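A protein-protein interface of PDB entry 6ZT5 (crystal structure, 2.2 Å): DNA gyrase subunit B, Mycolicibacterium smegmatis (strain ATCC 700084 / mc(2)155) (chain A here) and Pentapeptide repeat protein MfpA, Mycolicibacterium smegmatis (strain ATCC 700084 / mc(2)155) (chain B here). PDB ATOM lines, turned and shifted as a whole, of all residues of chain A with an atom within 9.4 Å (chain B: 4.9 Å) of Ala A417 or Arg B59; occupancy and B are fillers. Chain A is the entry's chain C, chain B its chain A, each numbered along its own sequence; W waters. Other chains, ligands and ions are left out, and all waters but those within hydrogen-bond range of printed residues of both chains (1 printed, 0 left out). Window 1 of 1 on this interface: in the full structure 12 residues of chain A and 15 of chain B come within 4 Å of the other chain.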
ATOM      1  N   ALA A 296     -33.573  -4.967  -3.951  1.00  0.00           N
ATOM      2  CA  ALA A 296     -34.029  -4.289  -5.186  1.00  0.00           C
ATOM      3  C   ALA A 296     -33.865  -2.774  -5.054  1.00  0.00           C
ATOM      4  O   ALA A 296     -33.943  -2.098  -6.077  1.00  0.00           O
ATOM      5  CB  ALA A 296     -35.468  -4.651  -5.439  1.00  0.00           C
ATOM      6  N   GLY A 297     -33.628  -2.275  -3.843  1.00  0.00           N
ATOM      7  CA  GLY A 297     -33.456  -0.839  -3.558  1.00  0.00           C
ATOM      8  C   GLY A 297     -32.166  -0.202  -4.089  1.00  0.00           C
ATOM      9  O   GLY A 297     -31.368  -0.858  -4.820  1.00  0.00           O
ATOM     10  N   TYR A 298     -31.941   1.053  -3.694  1.00  0.00           N
ATOM     11  CA  TYR A 298     -30.930   1.970  -4.276  1.00  0.00           C
ATOM     12  C   TYR A 298     -30.027   2.540  -3.180  1.00  0.00           C
ATOM     13  O   TYR A 298     -29.249   3.454  -3.486  1.00  0.00           O
ATOM     14  CB  TYR A 298     -31.649   3.008  -5.138  1.00  0.00           C
ATOM     15  CG  TYR A 298     -32.304   2.364  -6.333  1.00  0.00           C
ATOM     16  CD1 TYR A 298     -31.538   1.897  -7.377  1.00  0.00           C
ATOM     17  CD2 TYR A 298     -33.668   2.135  -6.385  1.00  0.00           C
ATOM     18  CE1 TYR A 298     -32.108   1.243  -8.455  1.00  0.00           C
ATOM     19  CE2 TYR A 298     -34.260   1.500  -7.465  1.00  0.00           C
ATOM     20  CZ  TYR A 298     -33.474   1.037  -8.495  1.00  0.00           C
ATOM     21  OH  TYR A 298     -34.031   0.398  -9.563  1.00  0.00           O
ATOM     22  N   LEU A 346     -17.012  -1.028 -13.209  1.00  0.00           N
ATOM     23  CA  LEU A 346     -18.089  -0.706 -12.248  1.00  0.00           C
ATOM     24  C   LEU A 346     -17.418  -0.009 -11.059  1.00  0.00           C
ATOM     25  O   LEU A 346     -16.281  -0.430 -10.710  1.00  0.00           O
ATOM     26  CB  LEU A 346     -18.795  -2.015 -11.876  1.00  0.00           C
ATOM     27  CG  LEU A 346     -19.456  -2.751 -13.044  1.00  0.00           C
ATOM     28  CD1 LEU A 346     -20.087  -4.039 -12.597  1.00  0.00           C
ATOM     29  CD2 LEU A 346     -20.493  -1.910 -13.760  1.00  0.00           C
ATOM     30  N   ASP A 349     -19.962   2.551  -5.679  1.00  0.00           N
ATOM     31  CA  ASP A 349     -21.347   3.099  -5.723  1.00  0.00           C
ATOM     32  C   ASP A 349     -22.235   2.176  -6.570  1.00  0.00           C
ATOM     33  O   ASP A 349     -23.318   1.827  -6.099  1.00  0.00           O
ATOM     34  CB  ASP A 349     -21.374   4.551  -6.205  1.00  0.00           C
ATOM     35  CG  ASP A 349     -20.730   5.550  -5.241  1.00  0.00           C
ATOM     36  OD1 ASP A 349     -20.663   5.262  -4.023  1.00  0.00           O
ATOM     37  OD2 ASP A 349     -20.307   6.617  -5.713  1.00  0.00           O
ATOM     38  N   ASP A 350     -21.775   1.706  -7.739  1.00  0.00           N
ATOM     39  CA  ASP A 350     -22.622   0.865  -8.628  1.00  0.00           C
ATOM     40  C   ASP A 350     -22.888  -0.487  -7.943  1.00  0.00           C
ATOM     41  O   ASP A 350     -24.026  -0.959  -8.007  1.00  0.00           O
ATOM     42  CB  ASP A 350     -22.005   0.721 -10.014  1.00  0.00           C
ATOM     43  CG  ASP A 350     -21.748   2.050 -10.719  1.00  0.00           C
ATOM     44  OD1 ASP A 350     -22.617   2.940 -10.616  1.00  0.00           O
ATOM     45  OD2 ASP A 350     -20.666   2.199 -11.306  1.00  0.00           O
ATOM     46  N   GLU A 353     -25.051  -0.498  -4.372  1.00  0.00           N
ATOM     47  CA  GLU A 353     -26.481  -0.147  -4.513  1.00  0.00           C
ATOM     48  C   GLU A 353     -27.333  -1.399  -4.251  1.00  0.00           C
ATOM     49  O   GLU A 353     -27.179  -2.420  -4.956  1.00  0.00           O
ATOM     50  CB  GLU A 353     -26.665   0.514  -5.869  1.00  0.00           C
ATOM     51  CG  GLU A 353     -28.075   0.930  -6.203  1.00  0.00           C
ATOM     52  CD  GLU A 353     -28.224   1.271  -7.677  1.00  0.00           C
ATOM     53  OE1 GLU A 353     -28.685   0.348  -8.478  1.00  0.00           O
ATOM     54  OE2 GLU A 353     -27.826   2.419  -8.025  1.00  0.00           O
ATOM     55  N   GLY A 354     -28.162  -1.328  -3.204  1.00  0.00           N
ATOM     56  CA  GLY A 354     -29.016  -2.423  -2.710  1.00  0.00           C
ATOM     57  C   GLY A 354     -28.263  -3.442  -1.872  1.00  0.00           C
ATOM     58  O   GLY A 354     -28.809  -4.517  -1.636  1.00  0.00           O
ATOM     59  N   ASN A 409     -26.080  -7.416 -13.257  1.00  0.00           N
ATOM     60  CA  ASN A 409     -26.963  -6.652 -14.179  1.00  0.00           C
ATOM     61  C   ASN A 409     -27.470  -5.412 -13.449  1.00  0.00           C
ATOM     62  O   ASN A 409     -27.486  -4.382 -14.050  1.00  0.00           O
ATOM     63  CB  ASN A 409     -28.083  -7.504 -14.785  1.00  0.00           C
ATOM     64  CG  ASN A 409     -27.579  -8.348 -15.943  1.00  0.00           C
ATOM     65  OD1 ASN A 409     -26.472  -8.135 -16.431  1.00  0.00           O
ATOM     66  ND2 ASN A 409     -28.369  -9.314 -16.385  1.00  0.00           N
ATOM     67  N   LYS A 410     -27.792  -5.516 -12.164  1.00  0.00           N
ATOM     68  CA  LYS A 410     -28.288  -4.370 -11.353  1.00  0.00           C
ATOM     69  C   LYS A 410     -27.185  -3.321 -11.306  1.00  0.00           C
ATOM     70  O   LYS A 410     -27.492  -2.159 -11.520  1.00  0.00           O
ATOM     71  CB  LYS A 410     -28.684  -4.823  -9.948  1.00  0.00           C
ATOM     72  CG  LYS A 410     -29.308  -3.751  -9.076  1.00  0.00           C
ATOM     73  CD  LYS A 410     -29.773  -4.289  -7.730  1.00  0.00           C
ATOM     74  CE  LYS A 410     -29.893  -3.203  -6.685  1.00  0.00           C
ATOM     75  NZ  LYS A 410     -30.860  -2.164  -7.100  1.00  0.00           N
ATOM     76  N   ALA A 411     -25.945  -3.743 -11.055  1.00  0.00           N
ATOM     77  CA  ALA A 411     -24.772  -2.847 -10.968  1.00  0.00           C
ATOM     78  C   ALA A 411     -24.424  -2.269 -12.356  1.00  0.00           C
ATOM     79  O   ALA A 411     -23.950  -1.133 -12.409  1.00  0.00           O
ATOM     80  CB  ALA A 411     -23.608  -3.589 -10.381  1.00  0.00           C
ATOM     81  N   VAL A 412     -24.624  -3.027 -13.436  1.00  0.00           N
ATOM     82  CA  VAL A 412     -24.313  -2.570 -14.828  1.00  0.00           C
ATOM     83  C   VAL A 412     -25.292  -1.455 -15.205  1.00  0.00           C
ATOM     84  O   VAL A 412     -24.836  -0.430 -15.694  1.00  0.00           O
ATOM     85  CB  VAL A 412     -24.369  -3.726 -15.837  1.00  0.00           C
ATOM     86  CG1 VAL A 412     -24.371  -3.226 -17.281  1.00  0.00           C
ATOM     87  CG2 VAL A 412     -23.228  -4.694 -15.595  1.00  0.00           C
ATOM     88  N   SER A 413     -26.587  -1.643 -14.946  1.00  0.00           N
ATOM     89  CA  SER A 413     -27.647  -0.658 -15.279  1.00  0.00           C
ATOM     90  C   SER A 413     -27.408   0.619 -14.446  1.00  0.00           C
ATOM     91  O   SER A 413     -27.589   1.747 -14.984  1.00  0.00           O
ATOM     92  CB  SER A 413     -29.024  -1.258 -15.087  1.00  0.00           C
ATOM     93  OG  SER A 413     -29.662  -0.678 -13.967  1.00  0.00           O
ATOM     94  N   SER A 414     -26.953   0.461 -13.197  1.00  0.00           N
ATOM     95  CA  SER A 414     -26.602   1.586 -12.297  1.00  0.00           C
ATOM     96  C   SER A 414     -25.416   2.359 -12.879  1.00  0.00           C
ATOM     97  O   SER A 414     -25.470   3.594 -12.891  1.00  0.00           O
ATOM     98  CB  SER A 414     -26.341   1.106 -10.900  1.00  0.00           C
ATOM     99  OG  SER A 414     -25.810   2.138 -10.079  1.00  0.00           O
ATOM    100  N   ALA A 415     -24.403   1.646 -13.388  1.00  0.00           N
ATOM    101  CA  ALA A 415     -23.147   2.209 -13.926  1.00  0.00           C
ATOM    102  C   ALA A 415     -23.442   3.033 -15.179  1.00  0.00           C
ATOM    103  O   ALA A 415     -22.826   4.098 -15.326  1.00  0.00           O
ATOM    104  CB  ALA A 415     -22.167   1.096 -14.209  1.00  0.00           C
ATOM    105  N   GLN A 416     -24.366   2.567 -16.015  1.00  0.00           N
ATOM    106  CA  GLN A 416     -24.799   3.234 -17.273  1.00  0.00           C
ATOM    107  C   GLN A 416     -25.583   4.508 -16.939  1.00  0.00           C
ATOM    108  O   GLN A 416     -25.400   5.513 -17.635  1.00  0.00           O
ATOM    109  CB  GLN A 416     -25.601   2.259 -18.132  1.00  0.00           C
ATOM    110  CG  GLN A 416     -24.720   1.174 -18.751  1.00  0.00           C
ATOM    111  CD  GLN A 416     -25.471   0.023 -19.381  1.00  0.00           C
ATOM    112  OE1 GLN A 416     -24.995  -0.626 -20.317  1.00  0.00           O
ATOM    113  NE2 GLN A 416     -26.646  -0.268 -18.841  1.00  0.00           N
ATOM    114  N   ALA A 417     -26.389   4.515 -15.878  1.00  0.00           N
ATOM    115  CA  ALA A 417     -27.151   5.724 -15.478  1.00  0.00           C
ATOM    116  C   ALA A 417     -26.170   6.725 -14.885  1.00  0.00           C
ATOM    117  O   ALA A 417     -26.276   7.907 -15.244  1.00  0.00           O
ATOM    118  CB  ALA A 417     -28.285   5.412 -14.526  1.00  0.00           C
ATOM    119  N   ARG A 418     -25.213   6.267 -14.072  1.00  0.00           N
ATOM    120  CA  ARG A 418     -24.243   7.191 -13.425  1.00  0.00           C
ATOM    121  C   ARG A 418     -23.347   7.837 -14.497  1.00  0.00           C
ATOM    122  O   ARG A 418     -23.126   9.073 -14.404  1.00  0.00           O
ATOM    123  CB  ARG A 418     -23.442   6.487 -12.329  1.00  0.00           C
ATOM    124  CG  ARG A 418     -22.650   7.434 -11.436  1.00  0.00           C
ATOM    125  CD  ARG A 418     -22.043   6.706 -10.242  1.00  0.00           C
ATOM    126  NE  ARG A 418     -22.913   5.595  -9.897  1.00  0.00           N
ATOM    127  CZ  ARG A 418     -23.817   5.609  -8.940  1.00  0.00           C
ATOM    128  NH1 ARG A 418     -23.940   6.663  -8.150  1.00  0.00           N
ATOM    129  NH2 ARG A 418     -24.572   4.543  -8.769  1.00  0.00           N
ATOM    130  N   ILE A 419     -22.868   7.083 -15.495  1.00  0.00           N
ATOM    131  CA  ILE A 419     -22.004   7.647 -16.600  1.00  0.00           C
ATOM    132  C   ILE A 419     -22.809   8.643 -17.454  1.00  0.00           C
ATOM    133  O   ILE A 419     -22.271   9.701 -17.735  1.00  0.00           O
ATOM    134  CB  ILE A 419     -21.358   6.532 -17.450  1.00  0.00           C
ATOM    135  CG1 ILE A 419     -20.377   5.699 -16.616  1.00  0.00           C
ATOM    136  CG2 ILE A 419     -20.681   7.076 -18.714  1.00  0.00           C
ATOM    137  CD1 ILE A 419     -20.030   4.345 -17.247  1.00  0.00           C
ATOM    138  N   ALA A 420     -24.052   8.329 -17.827  1.00  0.00           N
ATOM    139  CA  ALA A 420     -24.967   9.221 -18.586  1.00  0.00           C
ATOM    140  C   ALA A 420     -25.309  10.476 -17.762  1.00  0.00           C
ATOM    141  O   ALA A 420     -25.239  11.578 -18.304  1.00  0.00           O
ATOM    142  CB  ALA A 420     -26.208   8.469 -19.009  1.00  0.00           C
ATOM    143  N   ALA A 421     -25.615  10.346 -16.472  1.00  0.00           N
ATOM    144  CA  ALA A 421     -25.881  11.508 -15.590  1.00  0.00           C
ATOM    145  C   ALA A 421     -24.672  12.452 -15.608  1.00  0.00           C
ATOM    146  O   ALA A 421     -24.882  13.646 -15.799  1.00  0.00           O
ATOM    147  CB  ALA A 421     -26.223  11.071 -14.184  1.00  0.00           C
ATOM    148  N   ARG A 422     -23.454  11.932 -15.452  1.00  0.00           N
ATOM    149  CA  ARG A 422     -22.225  12.759 -15.334  1.00  0.00           C
ATOM    150  C   ARG A 422     -21.911  13.475 -16.666  1.00  0.00           C
ATOM    151  O   ARG A 422     -21.571  14.684 -16.629  1.00  0.00           O
ATOM    152  CB  ARG A 422     -21.065  11.891 -14.864  1.00  0.00           C
ATOM    153  CG  ARG A 422     -19.849  12.703 -14.464  1.00  0.00           C
ATOM    154  CD  ARG A 422     -18.823  11.877 -13.731  1.00  0.00           C
ATOM    155  NE  ARG A 422     -19.279  11.334 -12.453  1.00  0.00           N
ATOM    156  CZ  ARG A 422     -19.382  12.035 -11.319  1.00  0.00           C
ATOM    157  NH1 ARG A 422     -19.121  13.336 -11.302  1.00  0.00           N
ATOM    158  NH2 ARG A 422     -19.763  11.426 -10.208  1.00  0.00           N
ATOM    159  N   LYS A 423     -22.027  12.770 -17.795  1.00  0.00           N
ATOM    160  CA  LYS A 423     -21.778  13.316 -19.153  1.00  0.00           C
ATOM    161  C   LYS A 423     -22.750  14.486 -19.384  1.00  0.00           C
ATOM    162  O   LYS A 423     -22.325  15.486 -20.007  1.00  0.00           O
ATOM    163  CB  LYS A 423     -21.930  12.228 -20.230  1.00  0.00           C
ATOM    164  CG  LYS A 423     -20.643  11.776 -20.932  1.00  0.00           C
ATOM    165  CD  LYS A 423     -20.721  10.385 -21.627  1.00  0.00           C
ATOM    166  CE  LYS A 423     -19.629   9.403 -21.221  1.00  0.00           C
ATOM    167  NZ  LYS A 423     -19.847   8.028 -21.755  1.00  0.00           N
ATOM    168  N   ALA A 424     -24.005  14.367 -18.922  1.00  0.00           N
ATOM    169  CA  ALA A 424     -25.072  15.375 -19.159  1.00  0.00           C
ATOM    170  C   ALA A 424     -24.894  16.595 -18.230  1.00  0.00           C
ATOM    171  O   ALA A 424     -25.117  17.727 -18.703  1.00  0.00           O
ATOM    172  CB  ALA A 424     -26.441  14.745 -19.060  1.00  0.00           C
ATOM    173  N   ARG A 425     -24.426  16.390 -16.996  1.00  0.00           N
ATOM    174  CA  ARG A 425     -24.087  17.494 -16.060  1.00  0.00           C
ATOM    175  C   ARG A 425     -22.839  18.251 -16.548  1.00  0.00           C
ATOM    176  O   ARG A 425     -22.840  19.490 -16.400  1.00  0.00           O
ATOM    177  CB  ARG A 425     -23.908  16.978 -14.627  1.00  0.00           C
ATOM    178  CG  ARG A 425     -25.180  16.448 -13.977  1.00  0.00           C
ATOM    179  CD  ARG A 425     -26.326  17.447 -13.894  1.00  0.00           C
ATOM    180  NE  ARG A 425     -27.255  17.387 -15.020  1.00  0.00           N
ATOM    181  CZ  ARG A 425     -28.051  16.357 -15.333  1.00  0.00           C
ATOM    182  NH1 ARG A 425     -28.085  15.245 -14.605  1.00  0.00           N
ATOM    183  NH2 ARG A 425     -28.835  16.452 -16.393  1.00  0.00           N
ATOM    184  N   VAL B  37     -38.539   0.824 -13.651  1.00  0.00           N
ATOM    185  CA  VAL B  37     -37.307   1.568 -14.050  1.00  0.00           C
ATOM    186  C   VAL B  37     -37.652   2.418 -15.276  1.00  0.00           C
ATOM    187  O   VAL B  37     -37.906   1.839 -16.364  1.00  0.00           O
ATOM    188  CB  VAL B  37     -36.129   0.604 -14.306  1.00  0.00           C
ATOM    189  CG1 VAL B  37     -34.843   1.321 -14.709  1.00  0.00           C
ATOM    190  CG2 VAL B  37     -35.869  -0.277 -13.088  1.00  0.00           C
ATOM    191  N   PHE B  38     -37.703   3.741 -15.088  1.00  0.00           N
ATOM    192  CA  PHE B  38     -37.811   4.752 -16.171  1.00  0.00           C
ATOM    193  C   PHE B  38     -36.419   5.295 -16.489  1.00  0.00           C
ATOM    194  O   PHE B  38     -35.875   6.049 -15.666  1.00  0.00           O
ATOM    195  CB  PHE B  38     -38.722   5.901 -15.736  1.00  0.00           C
ATOM    196  CG  PHE B  38     -40.114   5.471 -15.351  1.00  0.00           C
ATOM    197  CD1 PHE B  38     -41.110   5.311 -16.306  1.00  0.00           C
ATOM    198  CD2 PHE B  38     -40.428   5.230 -14.028  1.00  0.00           C
ATOM    199  CE1 PHE B  38     -42.387   4.917 -15.935  1.00  0.00           C
ATOM    200  CE2 PHE B  38     -41.701   4.836 -13.657  1.00  0.00           C
ATOM    201  CZ  PHE B  38     -42.674   4.667 -14.610  1.00  0.00           C
ATOM    202  N   THR B  39     -35.871   4.934 -17.645  1.00  0.00           N
ATOM    203  CA  THR B  39     -34.527   5.356 -18.128  1.00  0.00           C
ATOM    204  C   THR B  39     -34.711   6.399 -19.245  1.00  0.00           C
ATOM    205  O   THR B  39     -35.391   6.080 -20.234  1.00  0.00           O
ATOM    206  CB  THR B  39     -33.735   4.130 -18.604  1.00  0.00           C
ATOM    207  OG1 THR B  39     -33.707   3.210 -17.515  1.00  0.00           O
ATOM    208  CG2 THR B  39     -32.338   4.468 -19.080  1.00  0.00           C
ATOM    209  N   GLU B  40     -34.156   7.599 -19.073  1.00  0.00           N
ATOM    210  CA  GLU B  40     -34.119   8.693 -20.087  1.00  0.00           C
ATOM    211  C   GLU B  40     -35.519   8.953 -20.662  1.00  0.00           C
ATOM    212  O   GLU B  40     -35.623   9.174 -21.878  1.00  0.00           O
ATOM    213  CB  GLU B  40     -33.122   8.364 -21.203  1.00  0.00           C
ATOM    214  CG  GLU B  40     -31.698   8.696 -20.823  1.00  0.00           C
ATOM    215  CD  GLU B  40     -30.602   7.909 -21.502  1.00  0.00           C
ATOM    216  OE1 GLU B  40     -30.767   6.690 -21.638  1.00  0.00           O
ATOM    217  OE2 GLU B  40     -29.579   8.516 -21.865  1.00  0.00           O
ATOM    218  N   CYS B  41     -36.546   8.919 -19.817  1.00  0.00           N
ATOM    219  CA  CYS B  41     -37.945   9.207 -20.196  1.00  0.00           C
ATOM    220  C   CYS B  41     -38.224  10.702 -20.011  1.00  0.00           C
ATOM    221  O   CYS B  41     -37.567  11.333 -19.187  1.00  0.00           O
ATOM    222  CB  CYS B  41     -38.923   8.359 -19.397  1.00  0.00           C
ATOM    223  SG  CYS B  41     -38.740   6.605 -19.789  1.00  0.00           S
ATOM    224  N   ALA B  57     -37.223   3.531 -10.214  1.00  0.00           N
ATOM    225  CA  ALA B  57     -36.066   4.338 -10.631  1.00  0.00           C
ATOM    226  C   ALA B  57     -36.522   5.298 -11.726  1.00  0.00           C
ATOM    227  O   ALA B  57     -37.149   4.847 -12.704  1.00  0.00           O
ATOM    228  CB  ALA B  57     -34.937   3.440 -11.059  1.00  0.00           C
ATOM    229  N   PHE B  58     -36.248   6.580 -11.527  1.00  0.00           N
ATOM    230  CA  PHE B  58     -36.436   7.645 -12.548  1.00  0.00           C
ATOM    231  C   PHE B  58     -35.048   8.187 -12.868  1.00  0.00           C
ATOM    232  O   PHE B  58     -34.607   9.113 -12.181  1.00  0.00           O
ATOM    233  CB  PHE B  58     -37.373   8.721 -11.991  1.00  0.00           C
ATOM    234  CG  PHE B  58     -38.701   8.188 -11.529  1.00  0.00           C
ATOM    235  CD1 PHE B  58     -38.840   7.654 -10.261  1.00  0.00           C
ATOM    236  CD2 PHE B  58     -39.797   8.188 -12.365  1.00  0.00           C
ATOM    237  CE1 PHE B  58     -40.052   7.121  -9.843  1.00  0.00           C
ATOM    238  CE2 PHE B  58     -41.018   7.696 -11.935  1.00  0.00           C
ATOM    239  CZ  PHE B  58     -41.143   7.160 -10.676  1.00  0.00           C
ATOM    240  N   ARG B  59     -34.327   7.553 -13.798  1.00  0.00           N
ATOM    241  CA  ARG B  59     -32.908   7.911 -14.008  1.00  0.00           C
ATOM    242  C   ARG B  59     -32.740   8.662 -15.319  1.00  0.00           C
ATOM    243  O   ARG B  59     -33.275   8.233 -16.336  1.00  0.00           O
ATOM    244  CB  ARG B  59     -32.001   6.691 -14.022  1.00  0.00           C
ATOM    245  CG  ARG B  59     -31.913   5.994 -12.671  1.00  0.00           C
ATOM    246  CD  ARG B  59     -31.890   4.528 -13.011  1.00  0.00           C
ATOM    247  NE  ARG B  59     -30.994   3.847 -12.153  1.00  0.00           N
ATOM    248  CZ  ARG B  59     -30.644   2.580 -12.296  1.00  0.00           C
ATOM    249  NH1 ARG B  59     -31.092   1.837 -13.299  1.00  0.00           N
ATOM    250  NH2 ARG B  59     -29.836   2.081 -11.394  1.00  0.00           N
ATOM    251  N   ASN B  60     -31.972   9.731 -15.241  1.00  0.00           N
ATOM    252  CA  ASN B  60     -31.663  10.663 -16.342  1.00  0.00           C
ATOM    253  C   ASN B  60     -32.978  11.024 -17.052  1.00  0.00           C
ATOM    254  O   ASN B  60     -32.951  11.130 -18.272  1.00  0.00           O
ATOM    255  CB  ASN B  60     -30.611  10.041 -17.264  1.00  0.00           C
ATOM    256  CG  ASN B  60     -29.316   9.795 -16.529  1.00  0.00           C
ATOM    257  OD1 ASN B  60     -28.707  10.742 -16.048  1.00  0.00           O
ATOM    258  ND2 ASN B  60     -28.889   8.543 -16.414  1.00  0.00           N
ATOM    259  N   CYS B  61     -34.083  11.163 -16.312  1.00  0.00           N
ATOM    260  CA  CYS B  61     -35.405  11.612 -16.828  1.00  0.00           C
ATOM    261  C   CYS B  61     -35.514  13.137 -16.696  1.00  0.00           C
ATOM    262  O   CYS B  61     -34.778  13.718 -15.889  1.00  0.00           O
ATOM    263  CB  CYS B  61     -36.553  10.953 -16.082  1.00  0.00           C
ATOM    264  SG  CYS B  61     -36.641   9.160 -16.340  1.00  0.00           S
ATOM    265  N   SER B  77     -34.868   5.722  -6.856  1.00  0.00           N
ATOM    266  CA  SER B  77     -33.729   6.451  -7.461  1.00  0.00           C
ATOM    267  C   SER B  77     -34.266   7.578  -8.331  1.00  0.00           C
ATOM    268  O   SER B  77     -35.199   7.319  -9.121  1.00  0.00           O
ATOM    269  CB  SER B  77     -32.818   5.556  -8.261  1.00  0.00           C
ATOM    270  OG  SER B  77     -31.744   6.342  -8.778  1.00  0.00           O
ATOM    271  N   LEU B  79     -31.664   9.403  -9.741  1.00  0.00           N
ATOM    272  CA  LEU B  79     -30.274   9.659 -10.200  1.00  0.00           C
ATOM    273  C   LEU B  79     -30.298  10.415 -11.545  1.00  0.00           C
ATOM    274  O   LEU B  79     -30.915   9.940 -12.496  1.00  0.00           O
ATOM    275  CB  LEU B  79     -29.531   8.324 -10.314  1.00  0.00           C
ATOM    276  CG  LEU B  79     -28.029   8.466 -10.540  1.00  0.00           C
ATOM    277  CD1 LEU B  79     -27.262   7.364  -9.833  1.00  0.00           C
ATOM    278  CD2 LEU B  79     -27.705   8.485 -12.011  1.00  0.00           C
ATOM    279  N   SER B  81     -31.812  12.953 -12.694  1.00  0.00           N
ATOM    280  CA  SER B  81     -33.065  13.529 -13.259  1.00  0.00           C
ATOM    281  C   SER B  81     -33.090  15.053 -13.081  1.00  0.00           C
ATOM    282  O   SER B  81     -32.396  15.568 -12.182  1.00  0.00           O
ATOM    283  CB  SER B  81     -34.302  12.848 -12.753  1.00  0.00           C
ATOM    284  OG  SER B  81     -34.434  11.552 -13.361  1.00  0.00           O
HETATM  285  O   HOH W   1     -29.466  -0.524 -11.025  1.00  0.00           O
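The side-chain carboxylate (OE1) of Glu A353 lies within salt-bridge range of the guanidinium group (NH2) of Arg B59 (3.6 Å). The guanidinium group (NH1) of Arg B59 sits at hydrogen-bond distance from the side-chain hydroxyl (OG) of Ser A413 (3.0 Å). The backbone carbonyl oxygen (O) of Ala A417 is in hydrogen-bond range of the side-chain amide nitrogen (ND2) of Asn B60, at 2.9 Å. The backbone NH (N) of Ala A421 lies close to the side-chain amide oxygen (OD1) of Asn B60, at 3.1 Å.
N of Phe B38 lies within hydrogen-bond range of O of Ala B57, at 2.7 Å. The backbone NH (N) of Glu B40 sits at hydrogen-bond distance from the backbone carbonyl oxygen (O) of Arg B59 (2.9 Å). The backbone NH (N) of Phe B58 sits at hydrogen-bond distance from the backbone carbonyl oxygen (O) of Ser B77 (2.7 Å). N of Leu B79 lies within hydrogen-bond range of OG of Ser B77 (3.2 Å). The side-chain carboxylate of Asp A350 lies within hydrogen-bond range of the side-chain hydroxyl of Ser A414 (3.3 Å). The side-chain carboxylate (OD1) of Asp A350 is in salt-bridge range of the guanidinium group (NE) of Arg A418 (2.8 Å).
Among the printed residues, merely in contact across the chains: Ser A414 with Arg B59 (3.4 Å), Tyr A298 with Ala B57 (3.5 Å), Ala A417 with Leu B79 (3.6 Å), Ala A421 with Leu B79 (3.7 Å), Ala A420 with Asn B60 (3.7 Å), Tyr A298 with Ser B77 (3.8 Å), Arg A418 with Leu B79 (3.8 Å), Tyr A298 with Arg B59 (3.8 Å) and Ala A417 with Arg B59 (3.9 Å).
Leu A346 touches none of the printed residues of chain B. Val A412 touches none of the printed residues of chain B. Of the printed residues of chain B, Ser A413 touches Arg B59. Of chain B, only Arg B59, Asn B60 and Leu B79 come within 4 Å of Ala A417. Of the printed residues of chain A, Ala B57 touches Tyr A298 (3.5 Å). Arg B59 touches five residues of chain A. The nearest residue of chain A that does not touch Arg B59 is Lys A410 (4.8 Å). The nearest printed residue of chain A that does not touch Ser B77 is Glu A353 (5.6 Å).
Of the 25 printed residues of chain A, 8 touch a printed residue of chain B. Printed residues of chain A that touch a printed residue of chain B: Tyr A298, Glu A353, Ser A413, Ser A414, Ala A417, Arg A418, Ala A420 and Ala A421. Of the 13 printed residues of chain B, 5 touch a printed residue of chain A. Printed residues of chain B that touch a printed residue of chain A: Ala B57, Arg B59, Asn B60, Ser B77 and Leu B79. Along chain B the printed residues that touch a printed residue of chain A span positions 57 to 79. Among the printed residues, 13 pairs touch across the chains. Among the printed residues, Asp or Glu carboxylates within 4 Å of a Lys or Arg side-chain nitrogen of the other chain: Glu A353 with Arg B59 (3.6 Å).
Water W1 lies within hydrogen-bond range of O of Lys A410 (2.6 Å), NH2 of Arg B59 (2.7 Å), OE1 of Glu A353 (2.8 Å), OG of Ser A413 (3.0 Å) and N of Ser A414 (3.5 Å).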
